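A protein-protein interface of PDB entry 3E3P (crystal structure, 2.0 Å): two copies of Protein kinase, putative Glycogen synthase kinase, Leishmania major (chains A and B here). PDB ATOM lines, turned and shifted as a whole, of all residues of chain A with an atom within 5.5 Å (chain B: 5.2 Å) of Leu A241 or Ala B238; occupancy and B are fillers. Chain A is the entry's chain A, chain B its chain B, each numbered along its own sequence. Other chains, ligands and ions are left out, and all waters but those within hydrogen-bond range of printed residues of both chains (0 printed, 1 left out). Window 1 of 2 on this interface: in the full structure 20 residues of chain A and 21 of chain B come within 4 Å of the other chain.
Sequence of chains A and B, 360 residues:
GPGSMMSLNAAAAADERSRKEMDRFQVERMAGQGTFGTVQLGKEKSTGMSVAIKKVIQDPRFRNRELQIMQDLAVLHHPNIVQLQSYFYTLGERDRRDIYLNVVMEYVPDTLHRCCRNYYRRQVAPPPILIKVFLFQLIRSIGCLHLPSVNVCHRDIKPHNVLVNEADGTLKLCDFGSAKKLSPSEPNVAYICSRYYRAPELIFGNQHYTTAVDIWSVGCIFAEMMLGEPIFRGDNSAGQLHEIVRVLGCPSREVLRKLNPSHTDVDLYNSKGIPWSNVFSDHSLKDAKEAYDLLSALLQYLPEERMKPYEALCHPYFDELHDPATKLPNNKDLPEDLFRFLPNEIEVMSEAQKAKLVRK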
ATOM      1  N   ILE A 203      20.395  12.287  12.794  1.00  0.00           N
ATOM      2  CA  ILE A 203      19.017  12.225  13.286  1.00  0.00           C
ATOM      3  C   ILE A 203      18.988  12.561  14.782  1.00  0.00           C
ATOM      4  O   ILE A 203      18.030  13.161  15.293  1.00  0.00           O
ATOM      5  CB  ILE A 203      18.377  10.828  13.037  1.00  0.00           C
ATOM      6  CG1 ILE A 203      18.351  10.532  11.531  1.00  0.00           C
ATOM      7  CG2 ILE A 203      16.940  10.751  13.637  1.00  0.00           C
ATOM      8  CD1 ILE A 203      17.954   9.106  11.202  1.00  0.00           C
ATOM      9  N   PHE A 204      20.040  12.156  15.483  1.00  0.00           N
ATOM     10  CA  PHE A 204      20.160  12.446  16.897  1.00  0.00           C
ATOM     11  C   PHE A 204      20.729  13.831  17.199  1.00  0.00           C
ATOM     12  O   PHE A 204      20.886  14.178  18.372  1.00  0.00           O
ATOM     13  CB  PHE A 204      21.011  11.384  17.589  1.00  0.00           C
ATOM     14  CG  PHE A 204      20.407  10.014  17.558  1.00  0.00           C
ATOM     15  CD1 PHE A 204      19.033   9.824  17.768  1.00  0.00           C
ATOM     16  CD2 PHE A 204      21.212   8.905  17.350  1.00  0.00           C
ATOM     17  CE1 PHE A 204      18.489   8.552  17.753  1.00  0.00           C
ATOM     18  CE2 PHE A 204      20.673   7.635  17.335  1.00  0.00           C
ATOM     19  CZ  PHE A 204      19.323   7.450  17.539  1.00  0.00           C
ATOM     20  N   ASN A 236       9.281  12.593   8.720  1.00  0.00           N
ATOM     21  CA  ASN A 236       9.790  13.490   9.738  1.00  0.00           C
ATOM     22  C   ASN A 236      10.983  12.824  10.391  1.00  0.00           C
ATOM     23  O   ASN A 236      11.335  11.702  10.044  1.00  0.00           O
ATOM     24  CB  ASN A 236       8.692  13.862  10.762  1.00  0.00           C
ATOM     25  CG  ASN A 236       7.789  12.691  11.115  1.00  0.00           C
ATOM     26  OD1 ASN A 236       8.240  11.692  11.662  1.00  0.00           O
ATOM     27  ND2 ASN A 236       6.497  12.819  10.813  1.00  0.00           N
ATOM     28  N   SER A 237      11.621  13.540  11.305  1.00  0.00           N
ATOM     29  CA  SER A 237      12.816  13.075  12.003  1.00  0.00           C
ATOM     30  C   SER A 237      12.542  11.808  12.815  1.00  0.00           C
ATOM     31  O   SER A 237      13.353  10.873  12.842  1.00  0.00           O
ATOM     32  CB  SER A 237      13.310  14.204  12.920  1.00  0.00           C
ATOM     33  OG  SER A 237      14.571  13.923  13.478  1.00  0.00           O
ATOM     34  N   ALA A 238      11.394  11.795  13.484  1.00  0.00           N
ATOM     35  CA  ALA A 238      10.984  10.651  14.283  1.00  0.00           C
ATOM     36  C   ALA A 238      10.728   9.469  13.343  1.00  0.00           C
ATOM     37  O   ALA A 238      11.246   8.372  13.564  1.00  0.00           O
ATOM     38  CB  ALA A 238       9.729  10.995  15.093  1.00  0.00           C
ATOM     39  N   GLY A 239       9.951   9.730  12.288  1.00  0.00           N
ATOM     40  CA  GLY A 239       9.689   8.764  11.225  1.00  0.00           C
ATOM     41  C   GLY A 239      10.939   8.229  10.546  1.00  0.00           C
ATOM     42  O   GLY A 239      10.976   7.073  10.122  1.00  0.00           O
ATOM     43  N   GLN A 240      11.961   9.064  10.424  1.00  0.00           N
ATOM     44  CA  GLN A 240      13.193   8.640   9.768  1.00  0.00           C
ATOM     45  C   GLN A 240      13.907   7.596  10.602  1.00  0.00           C
ATOM     46  O   GLN A 240      14.388   6.590  10.073  1.00  0.00           O
ATOM     47  CB  GLN A 240      14.111   9.831   9.513  1.00  0.00           C
ATOM     48  CG  GLN A 240      15.290   9.543   8.618  1.00  0.00           C
ATOM     49  CD  GLN A 240      14.907   9.106   7.212  1.00  0.00           C
ATOM     50  OE1 GLN A 240      13.875   9.532   6.640  1.00  0.00           O
ATOM     51  NE2 GLN A 240      15.752   8.256   6.634  1.00  0.00           N
ATOM     52  N   LEU A 241      13.973   7.840  11.909  1.00  0.00           N
ATOM     53  CA  LEU A 241      14.549   6.883  12.848  1.00  0.00           C
ATOM     54  C   LEU A 241      13.773   5.565  12.834  1.00  0.00           C
ATOM     55  O   LEU A 241      14.378   4.482  12.844  1.00  0.00           O
ATOM     56  CB  LEU A 241      14.555   7.471  14.259  1.00  0.00           C
ATOM     57  CG  LEU A 241      15.098   6.549  15.349  1.00  0.00           C
ATOM     58  CD1 LEU A 241      16.574   6.120  15.075  1.00  0.00           C
ATOM     59  CD2 LEU A 241      14.934   7.224  16.693  1.00  0.00           C
ATOM     60  N   HIS A 242      12.443   5.691  12.804  1.00  0.00           N
ATOM     61  CA  HIS A 242      11.497   4.585  12.712  1.00  0.00           C
ATOM     62  C   HIS A 242      11.812   3.652  11.550  1.00  0.00           C
ATOM     63  O   HIS A 242      11.917   2.427  11.740  1.00  0.00           O
ATOM     64  CB  HIS A 242      10.073   5.156  12.563  1.00  0.00           C
ATOM     65  CG  HIS A 242       8.997   4.122  12.408  1.00  0.00           C
ATOM     66  ND1 HIS A 242       8.026   3.909  13.366  1.00  0.00           N
ATOM     67  CD2 HIS A 242       8.712   3.267  11.392  1.00  0.00           C
ATOM     68  CE1 HIS A 242       7.209   2.954  12.958  1.00  0.00           C
ATOM     69  NE2 HIS A 242       7.603   2.548  11.764  1.00  0.00           N
ATOM     70  N   GLU A 243      11.971   4.230  10.358  1.00  0.00           N
ATOM     71  CA  GLU A 243      12.197   3.445   9.147  1.00  0.00           C
ATOM     72  C   GLU A 243      13.551   2.737   9.154  1.00  0.00           C
ATOM     73  O   GLU A 243      13.660   1.645   8.630  1.00  0.00           O
ATOM     74  CB  GLU A 243      12.053   4.317   7.902  1.00  0.00           C
ATOM     75  CG  GLU A 243      10.610   4.845   7.672  1.00  0.00           C
ATOM     76  CD  GLU A 243       9.580   3.729   7.523  1.00  0.00           C
ATOM     77  OE1 GLU A 243       9.881   2.713   6.857  1.00  0.00           O
ATOM     78  OE2 GLU A 243       8.458   3.865   8.062  1.00  0.00           O
ATOM     79  N   ILE A 244      14.561   3.357   9.755  1.00  0.00           N
ATOM     80  CA  ILE A 244      15.885   2.739   9.876  1.00  0.00           C
ATOM     81  C   ILE A 244      15.811   1.565  10.851  1.00  0.00           C
ATOM     82  O   ILE A 244      16.291   0.480  10.552  1.00  0.00           O
ATOM     83  CB  ILE A 244      16.926   3.746  10.365  1.00  0.00           C
ATOM     84  CG1 ILE A 244      17.080   4.885   9.345  1.00  0.00           C
ATOM     85  CG2 ILE A 244      18.283   3.045  10.613  1.00  0.00           C
ATOM     86  CD1 ILE A 244      17.781   6.131   9.877  1.00  0.00           C
ATOM     87  N   VAL A 245      15.190   1.803  12.012  1.00  0.00           N
ATOM     88  CA  VAL A 245      15.070   0.798  13.088  1.00  0.00           C
ATOM     89  C   VAL A 245      14.208  -0.369  12.616  1.00  0.00           C
ATOM     90  O   VAL A 245      14.532  -1.535  12.854  1.00  0.00           O
ATOM     91  CB  VAL A 245      14.481   1.406  14.391  1.00  0.00           C
ATOM     92  CG1 VAL A 245      14.176   0.319  15.403  1.00  0.00           C
ATOM     93  CG2 VAL A 245      15.445   2.396  14.982  1.00  0.00           C
ATOM     94  N   ARG A 246      13.136  -0.032  11.909  1.00  0.00           N
ATOM     95  CA  ARG A 246      12.263  -1.024  11.299  1.00  0.00           C
ATOM     96  C   ARG A 246      13.001  -2.054  10.436  1.00  0.00           C
ATOM     97  O   ARG A 246      12.582  -3.205  10.372  1.00  0.00           O
ATOM     98  CB  ARG A 246      11.221  -0.318  10.451  1.00  0.00           C
ATOM     99  CG  ARG A 246      10.194  -1.216   9.867  1.00  0.00           C
ATOM    100  CD  ARG A 246       9.125  -0.397   9.182  1.00  0.00           C
ATOM    101  NE  ARG A 246       8.299  -1.247   8.335  1.00  0.00           N
ATOM    102  CZ  ARG A 246       8.688  -1.764   7.168  1.00  0.00           C
ATOM    103  NH1 ARG A 246       9.904  -1.526   6.674  1.00  0.00           N
ATOM    104  NH2 ARG A 246       7.846  -2.535   6.485  1.00  0.00           N
ATOM    105  N   TYR A 269      12.951   1.093  20.914  1.00  0.00           N
ATOM    106  CA  TYR A 269      13.515   0.843  19.578  1.00  0.00           C
ATOM    107  C   TYR A 269      13.360  -0.654  19.276  1.00  0.00           C
ATOM    108  O   TYR A 269      14.292  -1.299  18.782  1.00  0.00           O
ATOM    109  CB  TYR A 269      15.005   1.209  19.507  1.00  0.00           C
ATOM    110  CG  TYR A 269      15.378   2.593  19.981  1.00  0.00           C
ATOM    111  CD1 TYR A 269      15.103   3.725  19.206  1.00  0.00           C
ATOM    112  CD2 TYR A 269      16.051   2.771  21.188  1.00  0.00           C
ATOM    113  CE1 TYR A 269      15.467   5.003  19.642  1.00  0.00           C
ATOM    114  CE2 TYR A 269      16.418   4.039  21.631  1.00  0.00           C
ATOM    115  CZ  TYR A 269      16.128   5.150  20.860  1.00  0.00           C
ATOM    116  OH  TYR A 269      16.499   6.397  21.319  1.00  0.00           O
ATOM    117  N   ASN B 236      16.594  15.878  20.814  1.00  0.00           N
ATOM    118  CA  ASN B 236      16.251  15.958  19.403  1.00  0.00           C
ATOM    119  C   ASN B 236      14.764  15.680  19.246  1.00  0.00           C
ATOM    120  O   ASN B 236      14.106  15.353  20.232  1.00  0.00           O
ATOM    121  CB  ASN B 236      17.093  14.977  18.585  1.00  0.00           C
ATOM    122  CG  ASN B 236      17.373  13.672  19.321  1.00  0.00           C
ATOM    123  OD1 ASN B 236      16.527  12.787  19.397  1.00  0.00           O
ATOM    124  ND2 ASN B 236      18.584  13.538  19.827  1.00  0.00           N
ATOM    125  N   SER B 237      14.245  15.836  18.024  1.00  0.00           N
ATOM    126  CA  SER B 237      12.834  15.577  17.718  1.00  0.00           C
ATOM    127  C   SER B 237      12.428  14.138  17.996  1.00  0.00           C
ATOM    128  O   SER B 237      11.344  13.871  18.518  1.00  0.00           O
ATOM    129  CB  SER B 237      12.531  15.891  16.247  1.00  0.00           C
ATOM    130  OG  SER B 237      12.232  17.264  16.066  1.00  0.00           O
ATOM    131  N   ALA B 238      13.294  13.206  17.612  1.00  0.00           N
ATOM    132  CA  ALA B 238      13.053  11.807  17.899  1.00  0.00           C
ATOM    133  C   ALA B 238      13.047  11.601  19.411  1.00  0.00           C
ATOM    134  O   ALA B 238      12.164  10.919  19.936  1.00  0.00           O
ATOM    135  CB  ALA B 238      14.108  10.922  17.230  1.00  0.00           C
ATOM    136  N   GLY B 239      14.030  12.198  20.092  1.00  0.00           N
ATOM    137  CA  GLY B 239      14.176  12.094  21.557  1.00  0.00           C
ATOM    138  C   GLY B 239      13.005  12.681  22.319  1.00  0.00           C
ATOM    139  O   GLY B 239      12.657  12.232  23.394  1.00  0.00           O
ATOM    140  N   GLN B 240      12.389  13.695  21.750  1.00  0.00           N
ATOM    141  CA  GLN B 240      11.221  14.295  22.354  1.00  0.00           C
ATOM    142  C   GLN B 240      10.045  13.311  22.341  1.00  0.00           C
ATOM    143  O   GLN B 240       9.281  13.232  23.308  1.00  0.00           O
ATOM    144  CB  GLN B 240      10.899  15.593  21.632  1.00  0.00           C
ATOM    145  CG  GLN B 240       9.813  16.445  22.282  1.00  0.00           C
ATOM    146  CD  GLN B 240      10.161  16.878  23.692  1.00  0.00           C
ATOM    147  OE1 GLN B 240      11.343  16.982  24.068  1.00  0.00           O
ATOM    148  NE2 GLN B 240       9.130  17.115  24.492  1.00  0.00           N
ATOM    149  N   LEU B 241       9.892  12.554  21.251  1.00  0.00           N
ATOM    150  CA  LEU B 241       8.854  11.524  21.187  1.00  0.00           C
ATOM    151  C   LEU B 241       9.194  10.386  22.137  1.00  0.00           C
ATOM    152  O   LEU B 241       8.331   9.892  22.853  1.00  0.00           O
ATOM    153  CB  LEU B 241       8.669  10.997  19.759  1.00  0.00           C
ATOM    154  CG  LEU B 241       7.435  10.108  19.545  1.00  0.00           C
ATOM    155  CD1 LEU B 241       6.125  10.845  19.869  1.00  0.00           C
ATOM    156  CD2 LEU B 241       7.424   9.581  18.102  1.00  0.00           C
ATOM    157  N   HIS B 242      10.463   9.988  22.149  1.00  0.00           N
ATOM    158  CA  HIS B 242      10.950   8.937  23.034  1.00  0.00           C
ATOM    159  C   HIS B 242      10.532   9.199  24.494  1.00  0.00           C
ATOM    160  O   HIS B 242       9.976   8.327  25.158  1.00  0.00           O
ATOM    161  CB  HIS B 242      12.474   8.853  22.903  1.00  0.00           C
ATOM    162  CG  HIS B 242      13.105   7.748  23.686  1.00  0.00           C
ATOM    163  ND1 HIS B 242      13.356   7.840  25.040  1.00  0.00           N
ATOM    164  CD2 HIS B 242      13.590   6.544  23.293  1.00  0.00           C
ATOM    165  CE1 HIS B 242      13.948   6.733  25.452  1.00  0.00           C
ATOM    166  NE2 HIS B 242      14.102   5.930  24.412  1.00  0.00           N
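Among the printed residues, merely in contact across the chains: Tyr A269 with His B242, Ser A237 with Ser B237, Leu A241 with Ala B238 and Ile A203 with Asn B236.
The side-chain amide nitrogen (ND2) of Asn B236 sits at hydrogen-bond distance from the backbone carbonyl oxygen (O) of Phe A204 (2.8 Å).
Of chain B, only Ala B238 comes within 4 Å of Leu A241. Of chain A, only Leu A241 (3.8 Å) comes within 4 Å of Ala B238. Of the printed residues of chain A, Ser B237 touches Ser A237. Printed residues of chain A within 4 Å of His B242: Tyr A269. Printed residues of chain B within 4 Å of Ser A237: Ser B237. Glu A243 touches none of the printed residues of chain B. Gly B239 touches none of the printed residues of chain A. The nearest printed residue of chain B that does not touch Leu A241 is Gly B239 (6.1 Å). The nearest printed residue of chain B that does not touch Tyr A269 is Gly B239 (6.2 Å).
Ser B237 touches its own counterpart, Ser A237. Leu A241 touches Ala B238, but with the chains exchanged Ala A238 does not touch Leu B241 (4.05 Å). 7 positions are printed for both chains.
OD1 of Asn B236 sits at hydrogen-bond distance from N of Gly B239, at 2.7 Å.
Of the 7 printed residues of chain B, 4 touch a printed residue of chain A. Of the 14 printed residues of chain A, 5 touch a printed residue of chain B. Printed residues of chain A that touch a printed residue of chain B: Ile A203, Phe A204, Ser A237, Leu A241 and Tyr A269. Hydrophobic or aromatic side chains of chain A within 4 Å of the printed part of chain B: Phe A204, Leu A241 and Tyr A269.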
